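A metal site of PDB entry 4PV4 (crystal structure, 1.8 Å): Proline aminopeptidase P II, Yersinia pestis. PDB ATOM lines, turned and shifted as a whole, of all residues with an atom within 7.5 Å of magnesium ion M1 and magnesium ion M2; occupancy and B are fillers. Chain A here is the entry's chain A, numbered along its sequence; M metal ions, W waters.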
ATOM      1  N   TYR A 227      -3.252  23.420 -14.754  1.00  0.00           N
ATOM      2  CA  TYR A 227      -2.732  22.189 -15.353  1.00  0.00           C
ATOM      3  C   TYR A 227      -3.898  21.434 -15.985  1.00  0.00           C
ATOM      4  O   TYR A 227      -5.062  21.797 -15.730  1.00  0.00           O
ATOM      5  CB  TYR A 227      -2.065  21.312 -14.291  1.00  0.00           C
ATOM      6  CG  TYR A 227      -2.932  20.975 -13.112  1.00  0.00           C
ATOM      7  CD1 TYR A 227      -3.011  21.830 -12.026  1.00  0.00           C
ATOM      8  CD2 TYR A 227      -3.704  19.826 -13.093  1.00  0.00           C
ATOM      9  CE1 TYR A 227      -3.838  21.567 -10.962  1.00  0.00           C
ATOM     10  CE2 TYR A 227      -4.533  19.531 -11.996  1.00  0.00           C
ATOM     11  CZ  TYR A 227      -4.581  20.411 -10.942  1.00  0.00           C
ATOM     12  OH  TYR A 227      -5.389  20.189  -9.855  1.00  0.00           O
ATOM     13  N   ILE A 230      -7.634  16.134 -14.730  1.00  0.00           N
ATOM     14  CA  ILE A 230      -7.740  14.652 -14.780  1.00  0.00           C
ATOM     15  C   ILE A 230      -9.171  14.341 -14.354  1.00  0.00           C
ATOM     16  O   ILE A 230      -9.554  14.795 -13.255  1.00  0.00           O
ATOM     17  CB  ILE A 230      -6.816  14.059 -13.749  1.00  0.00           C
ATOM     18  CG1 ILE A 230      -5.383  14.296 -14.211  1.00  0.00           C
ATOM     19  CG2 ILE A 230      -7.114  12.555 -13.491  1.00  0.00           C
ATOM     20  CD1 ILE A 230      -4.423  14.305 -13.055  1.00  0.00           C
ATOM     21  N   ILE A 257     -11.055  13.126  -9.777  1.00  0.00           N
ATOM     22  CA  ILE A 257     -10.907  14.384 -10.432  1.00  0.00           C
ATOM     23  C   ILE A 257      -9.810  15.211  -9.782  1.00  0.00           C
ATOM     24  O   ILE A 257      -9.898  15.589  -8.566  1.00  0.00           O
ATOM     25  CB  ILE A 257     -12.229  15.196 -10.369  1.00  0.00           C
ATOM     26  CG1 ILE A 257     -13.350  14.398 -11.020  1.00  0.00           C
ATOM     27  CG2 ILE A 257     -12.006  16.537 -11.055  1.00  0.00           C
ATOM     28  CD1 ILE A 257     -14.651  15.183 -11.151  1.00  0.00           C
ATOM     29  N   ASP A 258      -8.823  15.567 -10.573  1.00  0.00           N
ATOM     30  CA  ASP A 258      -7.743  16.399 -10.102  1.00  0.00           C
ATOM     31  C   ASP A 258      -7.749  17.649 -10.960  1.00  0.00           C
ATOM     32  O   ASP A 258      -7.569  17.568 -12.209  1.00  0.00           O
ATOM     33  CB  ASP A 258      -6.434  15.619 -10.196  1.00  0.00           C
ATOM     34  CG  ASP A 258      -5.239  16.381  -9.620  1.00  0.00           C
ATOM     35  OD1 ASP A 258      -5.330  17.599  -9.259  1.00  0.00           O
ATOM     36  OD2 ASP A 258      -4.191  15.701  -9.358  1.00  0.00           O
ATOM     37  N   ALA A 259      -8.094  18.793 -10.336  1.00  0.00           N
ATOM     38  CA  ALA A 259      -8.281  20.021 -11.093  1.00  0.00           C
ATOM     39  C   ALA A 259      -8.022  21.212 -10.209  1.00  0.00           C
ATOM     40  O   ALA A 259      -8.257  21.160  -8.996  1.00  0.00           O
ATOM     41  CB  ALA A 259      -9.682  20.122 -11.662  1.00  0.00           C
ATOM     42  N   GLY A 260      -7.532  22.282 -10.818  1.00  0.00           N
ATOM     43  CA  GLY A 260      -7.199  23.478 -10.044  1.00  0.00           C
ATOM     44  C   GLY A 260      -7.064  24.677 -10.984  1.00  0.00           C
ATOM     45  O   GLY A 260      -6.570  24.529 -12.127  1.00  0.00           O
ATOM     46  N   GLY A 268      -4.376  26.692  -7.726  1.00  0.00           N
ATOM     47  CA  GLY A 268      -4.984  25.716  -6.835  1.00  0.00           C
ATOM     48  C   GLY A 268      -4.701  24.315  -7.381  1.00  0.00           C
ATOM     49  O   GLY A 268      -4.396  24.148  -8.581  1.00  0.00           O
ATOM     50  N   ASP A 269      -4.899  23.320  -6.540  1.00  0.00           N
ATOM     51  CA  ASP A 269      -4.697  21.947  -6.934  1.00  0.00           C
ATOM     52  C   ASP A 269      -5.430  21.056  -5.995  1.00  0.00           C
ATOM     53  O   ASP A 269      -4.972  20.844  -4.849  1.00  0.00           O
ATOM     54  CB  ASP A 269      -3.236  21.653  -6.842  1.00  0.00           C
ATOM     55  CG  ASP A 269      -2.836  20.316  -7.364  1.00  0.00           C
ATOM     56  OD1 ASP A 269      -3.672  19.489  -7.740  1.00  0.00           O
ATOM     57  OD2 ASP A 269      -1.585  20.090  -7.243  1.00  0.00           O
ATOM     58  N   ILE A 270      -6.618  20.621  -6.400  1.00  0.00           N
ATOM     59  CA  ILE A 270      -7.476  19.788  -5.532  1.00  0.00           C
ATOM     60  C   ILE A 270      -7.679  18.468  -6.245  1.00  0.00           C
ATOM     61  O   ILE A 270      -7.892  18.424  -7.459  1.00  0.00           O
ATOM     62  CB  ILE A 270      -8.826  20.453  -5.288  1.00  0.00           C
ATOM     63  CG1 ILE A 270      -8.606  21.731  -4.511  1.00  0.00           C
ATOM     64  CG2 ILE A 270      -9.796  19.515  -4.580  1.00  0.00           C
ATOM     65  CD1 ILE A 270      -9.863  22.563  -4.340  1.00  0.00           C
ATOM     66  N   THR A 271      -7.701  17.386  -5.446  1.00  0.00           N
ATOM     67  CA  THR A 271      -8.204  16.113  -5.961  1.00  0.00           C
ATOM     68  C   THR A 271      -9.330  15.683  -5.049  1.00  0.00           C
ATOM     69  O   THR A 271      -9.228  15.721  -3.811  1.00  0.00           O
ATOM     70  CB  THR A 271      -7.133  14.994  -6.036  1.00  0.00           C
ATOM     71  OG1 THR A 271      -5.998  15.456  -6.812  1.00  0.00           O
ATOM     72  CG2 THR A 271      -7.738  13.787  -6.671  1.00  0.00           C
ATOM     73  N   GLY A 349       4.768  11.100  -4.440  1.00  0.00           N
ATOM     74  CA  GLY A 349       4.974  11.863  -3.216  1.00  0.00           C
ATOM     75  C   GLY A 349       3.683  12.252  -2.524  1.00  0.00           C
ATOM     76  O   GLY A 349       2.632  12.421  -3.174  1.00  0.00           O
ATOM     77  N   LEU A 350       3.769  12.468  -1.215  1.00  0.00           N
ATOM     78  CA  LEU A 350       2.643  12.992  -0.457  1.00  0.00           C
ATOM     79  C   LEU A 350       2.331  14.443  -0.720  1.00  0.00           C
ATOM     80  O   LEU A 350       1.161  14.919  -0.576  1.00  0.00           O
ATOM     81  CB  LEU A 350       2.947  12.860   1.038  1.00  0.00           C
ATOM     82  CG  LEU A 350       1.825  13.280   1.970  1.00  0.00           C
ATOM     83  CD1 LEU A 350       0.552  12.453   1.896  1.00  0.00           C
ATOM     84  CD2 LEU A 350       2.306  13.180   3.399  1.00  0.00           C
ATOM     85  N   SER A 351       3.366  15.197  -1.061  1.00  0.00           N
ATOM     86  CA  SER A 351       3.253  16.645  -1.106  1.00  0.00           C
ATOM     87  C   SER A 351       4.229  17.249  -2.079  1.00  0.00           C
ATOM     88  O   SER A 351       5.381  16.754  -2.210  1.00  0.00           O
ATOM     89  CB  SER A 351       3.629  17.251   0.261  1.00  0.00           C
ATOM     90  OG  SER A 351       2.769  16.836   1.287  1.00  0.00           O
ATOM     91  N   HIS A 352       3.788  18.303  -2.759  1.00  0.00           N
ATOM     92  CA  HIS A 352       4.716  19.192  -3.508  1.00  0.00           C
ATOM     93  C   HIS A 352       4.401  20.662  -3.167  1.00  0.00           C
ATOM     94  O   HIS A 352       3.305  21.016  -2.795  1.00  0.00           O
ATOM     95  CB  HIS A 352       4.648  18.950  -5.040  1.00  0.00           C
ATOM     96  CG  HIS A 352       3.285  19.120  -5.603  1.00  0.00           C
ATOM     97  ND1 HIS A 352       2.746  20.350  -5.916  1.00  0.00           N
ATOM     98  CD2 HIS A 352       2.341  18.194  -5.919  1.00  0.00           C
ATOM     99  CE1 HIS A 352       1.515  20.179  -6.372  1.00  0.00           C
ATOM    100  NE2 HIS A 352       1.276  18.885  -6.444  1.00  0.00           N
ATOM    101  N   TRP A 353       5.397  21.510  -3.291  1.00  0.00           N
ATOM    102  CA  TRP A 353       5.220  22.917  -3.140  1.00  0.00           C
ATOM    103  C   TRP A 353       4.182  23.394  -4.126  1.00  0.00           C
ATOM    104  O   TRP A 353       4.075  22.823  -5.246  1.00  0.00           O
ATOM    105  CB  TRP A 353       6.556  23.658  -3.466  1.00  0.00           C
ATOM    106  CG  TRP A 353       7.753  23.228  -2.727  1.00  0.00           C
ATOM    107  CD1 TRP A 353       8.967  22.943  -3.292  1.00  0.00           C
ATOM    108  CD2 TRP A 353       7.921  23.037  -1.302  1.00  0.00           C
ATOM    109  NE1 TRP A 353       9.870  22.600  -2.332  1.00  0.00           N
ATOM    110  CE2 TRP A 353       9.253  22.598  -1.119  1.00  0.00           C
ATOM    111  CE3 TRP A 353       7.086  23.120  -0.206  1.00  0.00           C
ATOM    112  CZ2 TRP A 353       9.774  22.338   0.120  1.00  0.00           C
ATOM    113  CZ3 TRP A 353       7.614  22.822   1.075  1.00  0.00           C
ATOM    114  CH2 TRP A 353       8.951  22.428   1.198  1.00  0.00           C
ATOM    115  N   LEU A 354       3.508  24.480  -3.798  1.00  0.00           N
ATOM    116  CA  LEU A 354       2.440  25.069  -4.617  1.00  0.00           C
ATOM    117  C   LEU A 354       2.626  26.593  -4.667  1.00  0.00           C
ATOM    118  O   LEU A 354       3.015  27.218  -3.685  1.00  0.00           O
ATOM    119  CB  LEU A 354       1.072  24.714  -4.017  1.00  0.00           C
ATOM    120  CG  LEU A 354      -0.125  25.214  -4.771  1.00  0.00           C
ATOM    121  CD1 LEU A 354      -0.251  24.400  -6.020  1.00  0.00           C
ATOM    122  CD2 LEU A 354      -1.346  24.973  -3.927  1.00  0.00           C
ATOM    123  N   VAL A 358       2.043  24.830 -10.395  1.00  0.00           N
ATOM    124  CA  VAL A 358       1.483  23.734  -9.640  1.00  0.00           C
ATOM    125  C   VAL A 358       2.492  22.844  -8.989  1.00  0.00           C
ATOM    126  O   VAL A 358       2.351  22.581  -7.745  1.00  0.00           O
ATOM    127  CB  VAL A 358       0.394  22.989 -10.436  1.00  0.00           C
ATOM    128  CG1 VAL A 358       0.963  22.272 -11.641  1.00  0.00           C
ATOM    129  CG2 VAL A 358      -0.382  22.030  -9.496  1.00  0.00           C
ATOM    130  N   HIS A 359       3.569  22.464  -9.671  1.00  0.00           N
ATOM    131  CA  HIS A 359       4.661  21.821  -9.037  1.00  0.00           C
ATOM    132  C   HIS A 359       5.666  22.930  -8.731  1.00  0.00           C
ATOM    133  O   HIS A 359       6.514  23.264  -9.574  1.00  0.00           O
ATOM    134  CB  HIS A 359       5.275  20.707  -9.903  1.00  0.00           C
ATOM    135  CG  HIS A 359       4.393  19.503 -10.053  1.00  0.00           C
ATOM    136  ND1 HIS A 359       4.523  18.598 -11.082  1.00  0.00           N
ATOM    137  CD2 HIS A 359       3.314  19.129  -9.354  1.00  0.00           C
ATOM    138  CE1 HIS A 359       3.550  17.699 -10.995  1.00  0.00           C
ATOM    139  NE2 HIS A 359       2.813  17.989  -9.949  1.00  0.00           N
ATOM    140  N   LEU A 379       1.941  24.046   0.184  1.00  0.00           N
ATOM    141  CA  LEU A 379       2.133  22.698  -0.291  1.00  0.00           C
ATOM    142  C   LEU A 379       0.839  21.937  -0.385  1.00  0.00           C
ATOM    143  O   LEU A 379      -0.177  22.279   0.223  1.00  0.00           O
ATOM    144  CB  LEU A 379       3.135  21.918   0.548  1.00  0.00           C
ATOM    145  CG  LEU A 379       2.839  21.723   2.034  1.00  0.00           C
ATOM    146  CD1 LEU A 379       3.503  20.474   2.612  1.00  0.00           C
ATOM    147  CD2 LEU A 379       3.186  22.952   2.840  1.00  0.00           C
ATOM    148  N   THR A 380       0.854  20.916  -1.236  1.00  0.00           N
ATOM    149  CA  THR A 380      -0.270  20.035  -1.369  1.00  0.00           C
ATOM    150  C   THR A 380      -0.159  18.905  -0.333  1.00  0.00           C
ATOM    151  O   THR A 380       0.938  18.533   0.155  1.00  0.00           O
ATOM    152  CB  THR A 380      -0.380  19.449  -2.774  1.00  0.00           C
ATOM    153  OG1 THR A 380       0.728  18.562  -3.067  1.00  0.00           O
ATOM    154  CG2 THR A 380      -0.449  20.565  -3.838  1.00  0.00           C
ATOM    155  N   VAL A 381      -1.276  18.264  -0.075  1.00  0.00           N
ATOM    156  CA  VAL A 381      -1.301  17.058   0.734  1.00  0.00           C
ATOM    157  C   VAL A 381      -2.205  16.057  -0.007  1.00  0.00           C
ATOM    158  O   VAL A 381      -3.409  16.318  -0.134  1.00  0.00           O
ATOM    159  CB  VAL A 381      -1.894  17.306   2.134  1.00  0.00           C
ATOM    160  CG1 VAL A 381      -1.916  16.030   2.987  1.00  0.00           C
ATOM    161  CG2 VAL A 381      -1.191  18.498   2.819  1.00  0.00           C
ATOM    162  N   GLU A 382      -1.615  15.020  -0.584  1.00  0.00           N
ATOM    163  CA  GLU A 382      -2.244  14.237  -1.611  1.00  0.00           C
ATOM    164  C   GLU A 382      -1.970  12.746  -1.563  1.00  0.00           C
ATOM    165  O   GLU A 382      -1.587  12.125  -2.520  1.00  0.00           O
ATOM    166  CB  GLU A 382      -1.945  14.850  -2.977  1.00  0.00           C
ATOM    167  CG  GLU A 382      -0.486  14.882  -3.360  1.00  0.00           C
ATOM    168  CD  GLU A 382      -0.401  15.472  -4.750  1.00  0.00           C
ATOM    169  OE1 GLU A 382      -1.069  14.881  -5.620  1.00  0.00           O
ATOM    170  OE2 GLU A 382       0.207  16.519  -4.934  1.00  0.00           O
ATOM    171  N   ARG A 403      -7.549   9.344  -4.832  1.00  0.00           N
ATOM    172  CA  ARG A 403      -6.659  10.303  -4.286  1.00  0.00           C
ATOM    173  C   ARG A 403      -7.528  11.393  -3.671  1.00  0.00           C
ATOM    174  O   ARG A 403      -8.585  11.760  -4.190  1.00  0.00           O
ATOM    175  CB  ARG A 403      -5.703  10.830  -5.397  1.00  0.00           C
ATOM    176  CG  ARG A 403      -4.843  11.991  -4.905  1.00  0.00           C
ATOM    177  CD  ARG A 403      -3.702  12.485  -5.750  1.00  0.00           C
ATOM    178  NE  ARG A 403      -4.088  12.961  -7.089  1.00  0.00           N
ATOM    179  CZ  ARG A 403      -4.098  12.266  -8.205  1.00  0.00           C
ATOM    180  NH1 ARG A 403      -4.405  12.883  -9.326  1.00  0.00           N
ATOM    181  NH2 ARG A 403      -3.789  10.988  -8.264  1.00  0.00           N
ATOM    182  N   GLU A 405      -6.813  15.327  -2.097  1.00  0.00           N
ATOM    183  CA  GLU A 405      -5.734  16.343  -2.086  1.00  0.00           C
ATOM    184  C   GLU A 405      -6.251  17.700  -1.726  1.00  0.00           C
ATOM    185  O   GLU A 405      -7.225  18.191  -2.387  1.00  0.00           O
ATOM    186  CB  GLU A 405      -5.112  16.442  -3.464  1.00  0.00           C
ATOM    187  CG  GLU A 405      -4.106  17.564  -3.593  1.00  0.00           C
ATOM    188  CD  GLU A 405      -3.424  17.574  -4.940  1.00  0.00           C
ATOM    189  OE1 GLU A 405      -3.941  16.975  -5.891  1.00  0.00           O
ATOM    190  OE2 GLU A 405      -2.299  18.130  -5.037  1.00  0.00           O
ATOM    191  N   ASP A 406      -5.664  18.296  -0.711  1.00  0.00           N
ATOM    192  CA  ASP A 406      -5.944  19.683  -0.309  1.00  0.00           C
ATOM    193  C   ASP A 406      -4.632  20.479  -0.451  1.00  0.00           C
ATOM    194  O   ASP A 406      -3.523  19.866  -0.541  1.00  0.00           O
ATOM    195  CB  ASP A 406      -6.390  19.767   1.148  1.00  0.00           C
ATOM    196  CG  ASP A 406      -7.848  19.428   1.325  1.00  0.00           C
ATOM    197  OD1 ASP A 406      -8.644  19.641   0.378  1.00  0.00           O
ATOM    198  OD2 ASP A 406      -8.165  18.951   2.455  1.00  0.00           O
ATOM    199  N   ASP A 407      -4.759  21.787  -0.398  1.00  0.00           N
ATOM    200  CA  ASP A 407      -3.634  22.761  -0.473  1.00  0.00           C
ATOM    201  C   ASP A 407      -3.579  23.457   0.901  1.00  0.00           C
ATOM    202  O   ASP A 407      -4.636  23.972   1.398  1.00  0.00           O
ATOM    203  CB  ASP A 407      -3.880  23.795  -1.529  1.00  0.00           C
ATOM    204  CG  ASP A 407      -4.134  23.187  -2.881  1.00  0.00           C
ATOM    205  OD1 ASP A 407      -3.621  22.079  -3.118  1.00  0.00           O
ATOM    206  OD2 ASP A 407      -4.891  23.831  -3.678  1.00  0.00           O
HETATM  207 MG    MG M   1      -3.375  17.430  -8.003  1.00  0.00          MG
HETATM  208 MG    MG M   2      -0.802  18.076  -6.496  1.00  0.00          MG
HETATM  209  O   HOH W   1      -1.348  16.520  -7.699  1.00  0.00           O
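The side-chain carboxylate of Asp 258 lies close to the guanidinium group of Arg 403 (2.8 Å).
The side-chain carboxylate (OD1) of Asp 258 sits close to the side-chain hydroxyl (OH) of Tyr 227 (2.7 Å).
ND1 of His 352 sits close to O of Val 358 (2.9 Å).
The side-chain hydroxyl (OH) of Tyr 227 lies within hydrogen-bond range of the backbone NH (N) of Gly 260 (3.1 Å).
The side-chain hydroxyl (OG1) of Thr 271 lies close to the side-chain carboxylate (OD2) of Asp 258 (3.1 Å).
O of His 352 sits at hydrogen-bond distance from N of Thr 380, 2.9 Å away.
O of Leu 350 sits at hydrogen-bond distance from N of Glu 382 (2.8 Å).
The backbone NH of Asp 269 is in hydrogen-bond range of the side-chain carboxylate of Asp 407 (2.9 Å).
Residues that only touch magnesium ion M1: Thr 271 (3.5 Å) and Tyr 227 (3.9 Å).
Within 4 Å of magnesium ion M1: Tyr 227, Asp 258, Asp 269, Thr 271 and Glu 405.
Along chain A the residues within 4 Å of magnesium ion M1 span positions 227 to 405.
CG2 of Thr 380 touches magnesium ion M2, 3.7 Å away.
Five residues have an atom within 4 Å of magnesium ion M2: Asp 269, His 352, Thr 380, Glu 382 and Glu 405.
The side-chain carboxylate (OD1) of Asp 269 binds magnesium ion M1, at 2.1 Å.
Magnesium ion M1 is bound by OE1 of Glu 405, at 2.2 Å.
Water W1 is bound to magnesium ion M1 (2.2 Å).
OD1 of Asp 258 is bound to magnesium ion M1 (2.3 Å).
The side-chain carboxylate (OD2) of Asp 258 is bound to magnesium ion M1, 2.3 Å away.
Magnesium ion M1 has five donor atoms within binding distance.
Magnesium ion M2 is bound by water W1, the side-chain carboxylate (OE2) of Glu 405, a ring nitrogen (NE2) of His 352, the side-chain carboxylate (OD2) of Asp 269 and the side-chain carboxylate (OE2) of Glu 382.
Magnesium ion M2 has five donor atoms within binding distance.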
